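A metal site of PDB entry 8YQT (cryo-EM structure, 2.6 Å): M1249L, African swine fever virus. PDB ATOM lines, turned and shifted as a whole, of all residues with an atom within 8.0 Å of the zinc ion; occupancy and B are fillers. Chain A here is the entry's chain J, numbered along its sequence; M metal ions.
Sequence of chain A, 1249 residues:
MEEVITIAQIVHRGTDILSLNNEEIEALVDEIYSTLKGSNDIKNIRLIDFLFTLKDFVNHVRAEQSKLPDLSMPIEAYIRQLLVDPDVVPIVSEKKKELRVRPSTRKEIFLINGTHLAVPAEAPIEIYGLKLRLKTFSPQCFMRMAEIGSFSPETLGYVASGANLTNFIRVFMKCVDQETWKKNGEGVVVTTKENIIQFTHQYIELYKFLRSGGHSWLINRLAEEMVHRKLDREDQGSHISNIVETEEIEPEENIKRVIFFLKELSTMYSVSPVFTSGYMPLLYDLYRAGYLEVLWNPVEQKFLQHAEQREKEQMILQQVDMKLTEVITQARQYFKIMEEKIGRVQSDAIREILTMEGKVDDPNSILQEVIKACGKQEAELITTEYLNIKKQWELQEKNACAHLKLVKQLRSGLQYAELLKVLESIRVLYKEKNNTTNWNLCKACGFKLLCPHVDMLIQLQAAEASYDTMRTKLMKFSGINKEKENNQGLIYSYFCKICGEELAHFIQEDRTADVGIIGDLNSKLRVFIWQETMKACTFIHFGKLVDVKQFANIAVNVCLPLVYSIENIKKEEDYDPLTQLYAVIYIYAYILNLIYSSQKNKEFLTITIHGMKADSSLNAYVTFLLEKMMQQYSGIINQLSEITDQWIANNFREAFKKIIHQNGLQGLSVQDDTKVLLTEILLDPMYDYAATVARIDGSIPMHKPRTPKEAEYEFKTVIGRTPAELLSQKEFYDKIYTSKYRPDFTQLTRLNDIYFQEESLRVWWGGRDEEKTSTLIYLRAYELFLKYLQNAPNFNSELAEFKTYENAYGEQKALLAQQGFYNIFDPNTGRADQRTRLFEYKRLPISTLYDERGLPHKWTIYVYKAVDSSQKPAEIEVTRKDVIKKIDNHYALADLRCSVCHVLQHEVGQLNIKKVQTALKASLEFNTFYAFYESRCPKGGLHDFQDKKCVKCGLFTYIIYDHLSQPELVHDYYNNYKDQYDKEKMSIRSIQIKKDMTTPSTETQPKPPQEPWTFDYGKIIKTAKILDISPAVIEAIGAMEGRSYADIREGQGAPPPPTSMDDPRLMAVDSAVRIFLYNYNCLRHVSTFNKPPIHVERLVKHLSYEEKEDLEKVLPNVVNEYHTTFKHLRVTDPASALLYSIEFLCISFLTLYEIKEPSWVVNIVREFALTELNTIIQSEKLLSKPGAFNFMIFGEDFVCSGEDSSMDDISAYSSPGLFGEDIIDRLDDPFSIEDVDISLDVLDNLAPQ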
ATOM      1  N   SER A 847      17.501 -23.760   4.201  1.00  0.00           N
ATOM      2  CA  SER A 847      17.975 -23.846   2.827  1.00  0.00           C
ATOM      3  C   SER A 847      19.486 -23.699   2.719  1.00  0.00           C
ATOM      4  O   SER A 847      20.039 -23.966   1.642  1.00  0.00           O
ATOM      5  CB  SER A 847      17.287 -22.780   1.968  1.00  0.00           C
ATOM      6  OG  SER A 847      17.734 -21.488   2.312  1.00  0.00           O
ATOM      7  N   LEU A 849      21.470 -25.658   4.153  1.00  0.00           N
ATOM      8  CA  LEU A 849      21.961 -27.019   4.201  1.00  0.00           C
ATOM      9  C   LEU A 849      21.276 -27.966   3.231  1.00  0.00           C
ATOM     10  O   LEU A 849      21.845 -29.006   2.923  1.00  0.00           O
ATOM     11  CB  LEU A 849      21.831 -27.593   5.623  1.00  0.00           C
ATOM     12  CG  LEU A 849      22.632 -26.951   6.749  1.00  0.00           C
ATOM     13  CD1 LEU A 849      22.276 -27.596   8.070  1.00  0.00           C
ATOM     14  CD2 LEU A 849      24.121 -27.073   6.480  1.00  0.00           C
ATOM     15  N   TYR A 850      20.068 -27.639   2.774  1.00  0.00           N
ATOM     16  CA  TYR A 850      19.307 -28.533   1.900  1.00  0.00           C
ATOM     17  C   TYR A 850      18.683 -27.727   0.777  1.00  0.00           C
ATOM     18  O   TYR A 850      18.441 -26.527   0.892  1.00  0.00           O
ATOM     19  CB  TYR A 850      18.224 -29.283   2.683  1.00  0.00           C
ATOM     20  CG  TYR A 850      18.782 -30.166   3.779  1.00  0.00           C
ATOM     21  CD1 TYR A 850      19.161 -31.472   3.529  1.00  0.00           C
ATOM     22  CD2 TYR A 850      18.958 -29.671   5.067  1.00  0.00           C
ATOM     23  CE1 TYR A 850      19.676 -32.267   4.520  1.00  0.00           C
ATOM     24  CE2 TYR A 850      19.475 -30.457   6.069  1.00  0.00           C
ATOM     25  CZ  TYR A 850      19.834 -31.755   5.795  1.00  0.00           C
ATOM     26  OH  TYR A 850      20.358 -32.536   6.793  1.00  0.00           O
ATOM     27  N   ASP A 851      18.434 -28.401  -0.340  1.00  0.00           N
ATOM     28  CA  ASP A 851      17.834 -27.774  -1.512  1.00  0.00           C
ATOM     29  C   ASP A 851      16.330 -28.020  -1.526  1.00  0.00           C
ATOM     30  O   ASP A 851      15.772 -28.672  -0.634  1.00  0.00           O
ATOM     31  CB  ASP A 851      18.505 -28.286  -2.781  1.00  0.00           C
ATOM     32  CG  ASP A 851      18.372 -29.788  -2.968  1.00  0.00           C
ATOM     33  OD1 ASP A 851      17.855 -30.461  -2.055  1.00  0.00           O
ATOM     34  OD2 ASP A 851      18.770 -30.294  -4.033  1.00  0.00           O
ATOM     35  N   GLU A 852      15.654 -27.492  -2.539  1.00  0.00           N
ATOM     36  CA  GLU A 852      14.211 -27.645  -2.678  1.00  0.00           C
ATOM     37  C   GLU A 852      13.779 -29.076  -2.944  1.00  0.00           C
ATOM     38  O   GLU A 852      12.579 -29.310  -3.098  1.00  0.00           O
ATOM     39  CB  GLU A 852      13.685 -26.734  -3.783  1.00  0.00           C
ATOM     40  CG  GLU A 852      13.738 -25.251  -3.448  1.00  0.00           C
ATOM     41  CD  GLU A 852      13.350 -24.375  -4.620  1.00  0.00           C
ATOM     42  OE1 GLU A 852      13.238 -24.907  -5.745  1.00  0.00           O
ATOM     43  OE2 GLU A 852      13.171 -23.159  -4.415  1.00  0.00           O
ATOM     44  N   ARG A 853      14.710 -30.019  -3.025  1.00  0.00           N
ATOM     45  CA  ARG A 853      14.386 -31.438  -3.159  1.00  0.00           C
ATOM     46  C   ARG A 853      14.795 -32.242  -1.931  1.00  0.00           C
ATOM     47  O   ARG A 853      14.744 -33.478  -1.972  1.00  0.00           O
ATOM     48  CB  ARG A 853      15.039 -32.018  -4.415  1.00  0.00           C
ATOM     49  CG  ARG A 853      14.463 -31.472  -5.709  1.00  0.00           C
ATOM     50  CD  ARG A 853      14.345 -32.554  -6.762  1.00  0.00           C
ATOM     51  NE  ARG A 853      15.653 -33.011  -7.206  1.00  0.00           N
ATOM     52  CZ  ARG A 853      16.066 -34.275  -7.144  1.00  0.00           C
ATOM     53  NH1 ARG A 853      15.285 -35.232  -6.687  1.00  0.00           N
ATOM     54  NH2 ARG A 853      17.293 -34.572  -7.562  1.00  0.00           N
ATOM     55  N   LEU A 855      17.813 -32.499  -0.474  1.00  0.00           N
ATOM     56  CA  LEU A 855      19.143 -33.078  -0.511  1.00  0.00           C
ATOM     57  C   LEU A 855      20.172 -32.097   0.053  1.00  0.00           C
ATOM     58  O   LEU A 855      20.041 -30.879  -0.133  1.00  0.00           O
ATOM     59  CB  LEU A 855      19.542 -33.453  -1.939  1.00  0.00           C
ATOM     60  CG  LEU A 855      18.629 -34.442  -2.663  1.00  0.00           C
ATOM     61  CD1 LEU A 855      19.004 -34.545  -4.139  1.00  0.00           C
ATOM     62  CD2 LEU A 855      18.677 -35.801  -2.002  1.00  0.00           C
ATOM     63  N   PRO A 856      21.192 -32.591   0.744  1.00  0.00           N
ATOM     64  CA  PRO A 856      22.228 -31.686   1.269  1.00  0.00           C
ATOM     65  C   PRO A 856      23.077 -31.117   0.152  1.00  0.00           C
ATOM     66  O   PRO A 856      23.199 -31.681  -0.935  1.00  0.00           O
ATOM     67  CB  PRO A 856      23.040 -32.593   2.198  1.00  0.00           C
ATOM     68  CG  PRO A 856      22.806 -33.955   1.705  1.00  0.00           C
ATOM     69  CD  PRO A 856      21.408 -33.980   1.164  1.00  0.00           C
ATOM     70  N   HIS A 857      23.682 -29.965   0.441  1.00  0.00           N
ATOM     71  CA  HIS A 857      24.579 -29.309  -0.505  1.00  0.00           C
ATOM     72  C   HIS A 857      25.973 -29.913  -0.429  1.00  0.00           C
ATOM     73  O   HIS A 857      26.440 -30.310   0.635  1.00  0.00           O
ATOM     74  CB  HIS A 857      24.646 -27.812  -0.239  1.00  0.00           C
ATOM     75  CG  HIS A 857      23.351 -27.095  -0.407  1.00  0.00           C
ATOM     76  ND1 HIS A 857      22.608 -27.155  -1.556  1.00  0.00           N
ATOM     77  CD2 HIS A 857      22.672 -26.268   0.432  1.00  0.00           C
ATOM     78  CE1 HIS A 857      21.520 -26.419  -1.417  1.00  0.00           C
ATOM     79  NE2 HIS A 857      21.536 -25.870  -0.217  1.00  0.00           N
ATOM     80  N   LYS A 858      26.630 -29.978  -1.588  1.00  0.00           N
ATOM     81  CA  LYS A 858      28.016 -30.422  -1.701  1.00  0.00           C
ATOM     82  C   LYS A 858      28.806 -29.292  -2.370  1.00  0.00           C
ATOM     83  O   LYS A 858      28.805 -29.166  -3.591  1.00  0.00           O
ATOM     84  CB  LYS A 858      28.124 -31.710  -2.504  1.00  0.00           C
ATOM     85  CG  LYS A 858      27.315 -32.873  -1.954  1.00  0.00           C
ATOM     86  CD  LYS A 858      27.963 -33.431  -0.707  1.00  0.00           C
ATOM     87  CE  LYS A 858      27.265 -34.700  -0.251  1.00  0.00           C
ATOM     88  NZ  LYS A 858      27.533 -35.829  -1.174  1.00  0.00           N
ATOM     89  N   TRP A 859      29.480 -28.476  -1.558  1.00  0.00           N
ATOM     90  CA  TRP A 859      30.198 -27.305  -2.073  1.00  0.00           C
ATOM     91  C   TRP A 859      31.584 -27.743  -2.544  1.00  0.00           C
ATOM     92  O   TRP A 859      32.617 -27.446  -1.935  1.00  0.00           O
ATOM     93  CB  TRP A 859      30.266 -26.210  -1.023  1.00  0.00           C
ATOM     94  CG  TRP A 859      28.926 -25.847  -0.449  1.00  0.00           C
ATOM     95  CD1 TRP A 859      28.490 -26.086   0.822  1.00  0.00           C
ATOM     96  CD2 TRP A 859      27.857 -25.188  -1.122  1.00  0.00           C
ATOM     97  NE1 TRP A 859      27.209 -25.618   0.973  1.00  0.00           N
ATOM     98  CE2 TRP A 859      26.800 -25.064  -0.204  1.00  0.00           C
ATOM     99  CE3 TRP A 859      27.686 -24.689  -2.418  1.00  0.00           C
ATOM    100  CZ2 TRP A 859      25.596 -24.454  -0.536  1.00  0.00           C
ATOM    101  CZ3 TRP A 859      26.486 -24.088  -2.753  1.00  0.00           C
ATOM    102  CH2 TRP A 859      25.453 -23.982  -1.814  1.00  0.00           C
ATOM    103  N   ARG A 897      30.031 -23.598  -5.853  1.00  0.00           N
ATOM    104  CA  ARG A 897      28.811 -24.113  -6.456  1.00  0.00           C
ATOM    105  C   ARG A 897      28.491 -25.487  -5.875  1.00  0.00           C
ATOM    106  O   ARG A 897      29.390 -26.281  -5.603  1.00  0.00           O
ATOM    107  CB  ARG A 897      28.943 -24.197  -7.976  1.00  0.00           C
ATOM    108  CG  ARG A 897      27.677 -24.637  -8.681  1.00  0.00           C
ATOM    109  CD  ARG A 897      27.831 -24.583 -10.182  1.00  0.00           C
ATOM    110  NE  ARG A 897      27.982 -23.219 -10.663  1.00  0.00           N
ATOM    111  CZ  ARG A 897      26.974 -22.423 -10.996  1.00  0.00           C
ATOM    112  NH1 ARG A 897      25.712 -22.817 -10.903  1.00  0.00           N
ATOM    113  NH2 ARG A 897      27.243 -21.192 -11.421  1.00  0.00           N
ATOM    114  N   CYS A 898      27.204 -25.743  -5.672  1.00  0.00           N
ATOM    115  CA  CYS A 898      26.772 -27.075  -5.259  1.00  0.00           C
ATOM    116  C   CYS A 898      26.860 -28.034  -6.437  1.00  0.00           C
ATOM    117  O   CYS A 898      26.551 -27.671  -7.580  1.00  0.00           O
ATOM    118  CB  CYS A 898      25.345 -27.022  -4.719  1.00  0.00           C
ATOM    119  SG  CYS A 898      24.728 -28.588  -4.072  1.00  0.00           S
ATOM    120  N   SER A 899      27.294 -29.256  -6.163  1.00  0.00           N
ATOM    121  CA  SER A 899      27.421 -30.285  -7.186  1.00  0.00           C
ATOM    122  C   SER A 899      26.176 -31.141  -7.312  1.00  0.00           C
ATOM    123  O   SER A 899      26.173 -32.104  -8.083  1.00  0.00           O
ATOM    124  CB  SER A 899      28.639 -31.159  -6.894  1.00  0.00           C
ATOM    125  OG  SER A 899      28.491 -31.855  -5.672  1.00  0.00           O
ATOM    126  N   VAL A 900      25.113 -30.826  -6.571  1.00  0.00           N
ATOM    127  CA  VAL A 900      23.860 -31.575  -6.610  1.00  0.00           C
ATOM    128  C   VAL A 900      22.741 -30.742  -7.217  1.00  0.00           C
ATOM    129  O   VAL A 900      22.151 -31.129  -8.236  1.00  0.00           O
ATOM    130  CB  VAL A 900      23.482 -32.095  -5.205  1.00  0.00           C
ATOM    131  CG1 VAL A 900      22.174 -32.853  -5.255  1.00  0.00           C
ATOM    132  CG2 VAL A 900      24.590 -32.964  -4.649  1.00  0.00           C
ATOM    133  N   CYS A 901      22.422 -29.607  -6.608  1.00  0.00           N
ATOM    134  CA  CYS A 901      21.380 -28.723  -7.112  1.00  0.00           C
ATOM    135  C   CYS A 901      21.924 -27.606  -8.002  1.00  0.00           C
ATOM    136  O   CYS A 901      21.120 -26.867  -8.587  1.00  0.00           O
ATOM    137  CB  CYS A 901      20.600 -28.105  -5.952  1.00  0.00           C
ATOM    138  SG  CYS A 901      21.543 -26.988  -4.904  1.00  0.00           S
ATOM    139  N   HIS A 902      23.241 -27.466  -8.103  1.00  0.00           N
ATOM    140  CA  HIS A 902      23.891 -26.496  -8.988  1.00  0.00           C
ATOM    141  C   HIS A 902      23.455 -25.065  -8.667  1.00  0.00           C
ATOM    142  O   HIS A 902      22.930 -24.345  -9.519  1.00  0.00           O
ATOM    143  CB  HIS A 902      23.634 -26.832 -10.453  1.00  0.00           C
ATOM    144  CG  HIS A 902      23.704 -28.291 -10.762  1.00  0.00           C
ATOM    145  ND1 HIS A 902      22.611 -29.035 -11.144  1.00  0.00           N
ATOM    146  CD2 HIS A 902      24.748 -29.160 -10.726  1.00  0.00           C
ATOM    147  CE1 HIS A 902      22.978 -30.283 -11.340  1.00  0.00           C
ATOM    148  NE2 HIS A 902      24.269 -30.395 -11.085  1.00  0.00           N
ATOM    149  N   VAL A 903      23.670 -24.664  -7.427  1.00  0.00           N
ATOM    150  CA  VAL A 903      23.370 -23.306  -6.990  1.00  0.00           C
ATOM    151  C   VAL A 903      24.647 -22.688  -6.427  1.00  0.00           C
ATOM    152  O   VAL A 903      25.471 -23.364  -5.795  1.00  0.00           O
ATOM    153  CB  VAL A 903      22.226 -23.263  -5.953  1.00  0.00           C
ATOM    154  CG1 VAL A 903      22.708 -23.662  -4.564  1.00  0.00           C
ATOM    155  CG2 VAL A 903      21.591 -21.886  -5.918  1.00  0.00           C
ATOM    156  N   VAL A 908      21.976 -18.887  -2.453  1.00  0.00           N
ATOM    157  CA  VAL A 908      21.199 -19.909  -1.747  1.00  0.00           C
ATOM    158  C   VAL A 908      19.967 -19.333  -1.080  1.00  0.00           C
ATOM    159  O   VAL A 908      19.038 -20.084  -0.756  1.00  0.00           O
ATOM    160  CB  VAL A 908      22.079 -20.645  -0.721  1.00  0.00           C
ATOM    161  CG1 VAL A 908      22.125 -19.902   0.600  1.00  0.00           C
ATOM    162  CG2 VAL A 908      21.594 -22.078  -0.522  1.00  0.00           C
ATOM    163  N   LEU A 911      16.324 -19.857  -2.735  1.00  0.00           N
ATOM    164  CA  LEU A 911      15.571 -21.089  -2.591  1.00  0.00           C
ATOM    165  C   LEU A 911      14.353 -20.855  -1.712  1.00  0.00           C
ATOM    166  O   LEU A 911      14.440 -20.185  -0.680  1.00  0.00           O
ATOM    167  CB  LEU A 911      16.438 -22.189  -1.982  1.00  0.00           C
ATOM    168  CG  LEU A 911      17.685 -22.614  -2.769  1.00  0.00           C
ATOM    169  CD1 LEU A 911      18.520 -23.575  -1.937  1.00  0.00           C
ATOM    170  CD2 LEU A 911      17.306 -23.241  -4.100  1.00  0.00           C
HETATM  171 ZN    ZN M   1      22.515 -28.461  -3.447  1.00  0.00          ZN
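The side-chain sulfur (SG) of Cys 901 is bound to the zinc ion, at 2.3 Å. ND1 of His 857 binds the zinc ion (2.3 Å). SG of Cys 898 binds the zinc ion (2.3 Å).
Of the 20 residues printed, 3 come within 4 Å of the zinc ion. The nearest printed residue that does not touch the zinc ion is Asp 851 (4.1 Å).
The side-chain sulfur (SG) of Cys 898 lies close to the backbone NH (N) of Lys 858, 3.4 Å away. The backbone NH of His 857 is in hydrogen-bond range of the backbone carbonyl oxygen of Leu 849, at 3.2 Å. NE2 of His 857 lies within hydrogen-bond range of O of Ser 847 (3.1 Å). The backbone NH (N) of Cys 898 is in hydrogen-bond range of the backbone carbonyl oxygen (O) of Val 903. The backbone carbonyl oxygen of Tyr 850 is in hydrogen-bond range of a ring nitrogen (NE2) of His 857. The side-chain sulfur (SG) of Cys 898 lies close to the backbone NH (N) of Val 900, 3.4 Å away.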
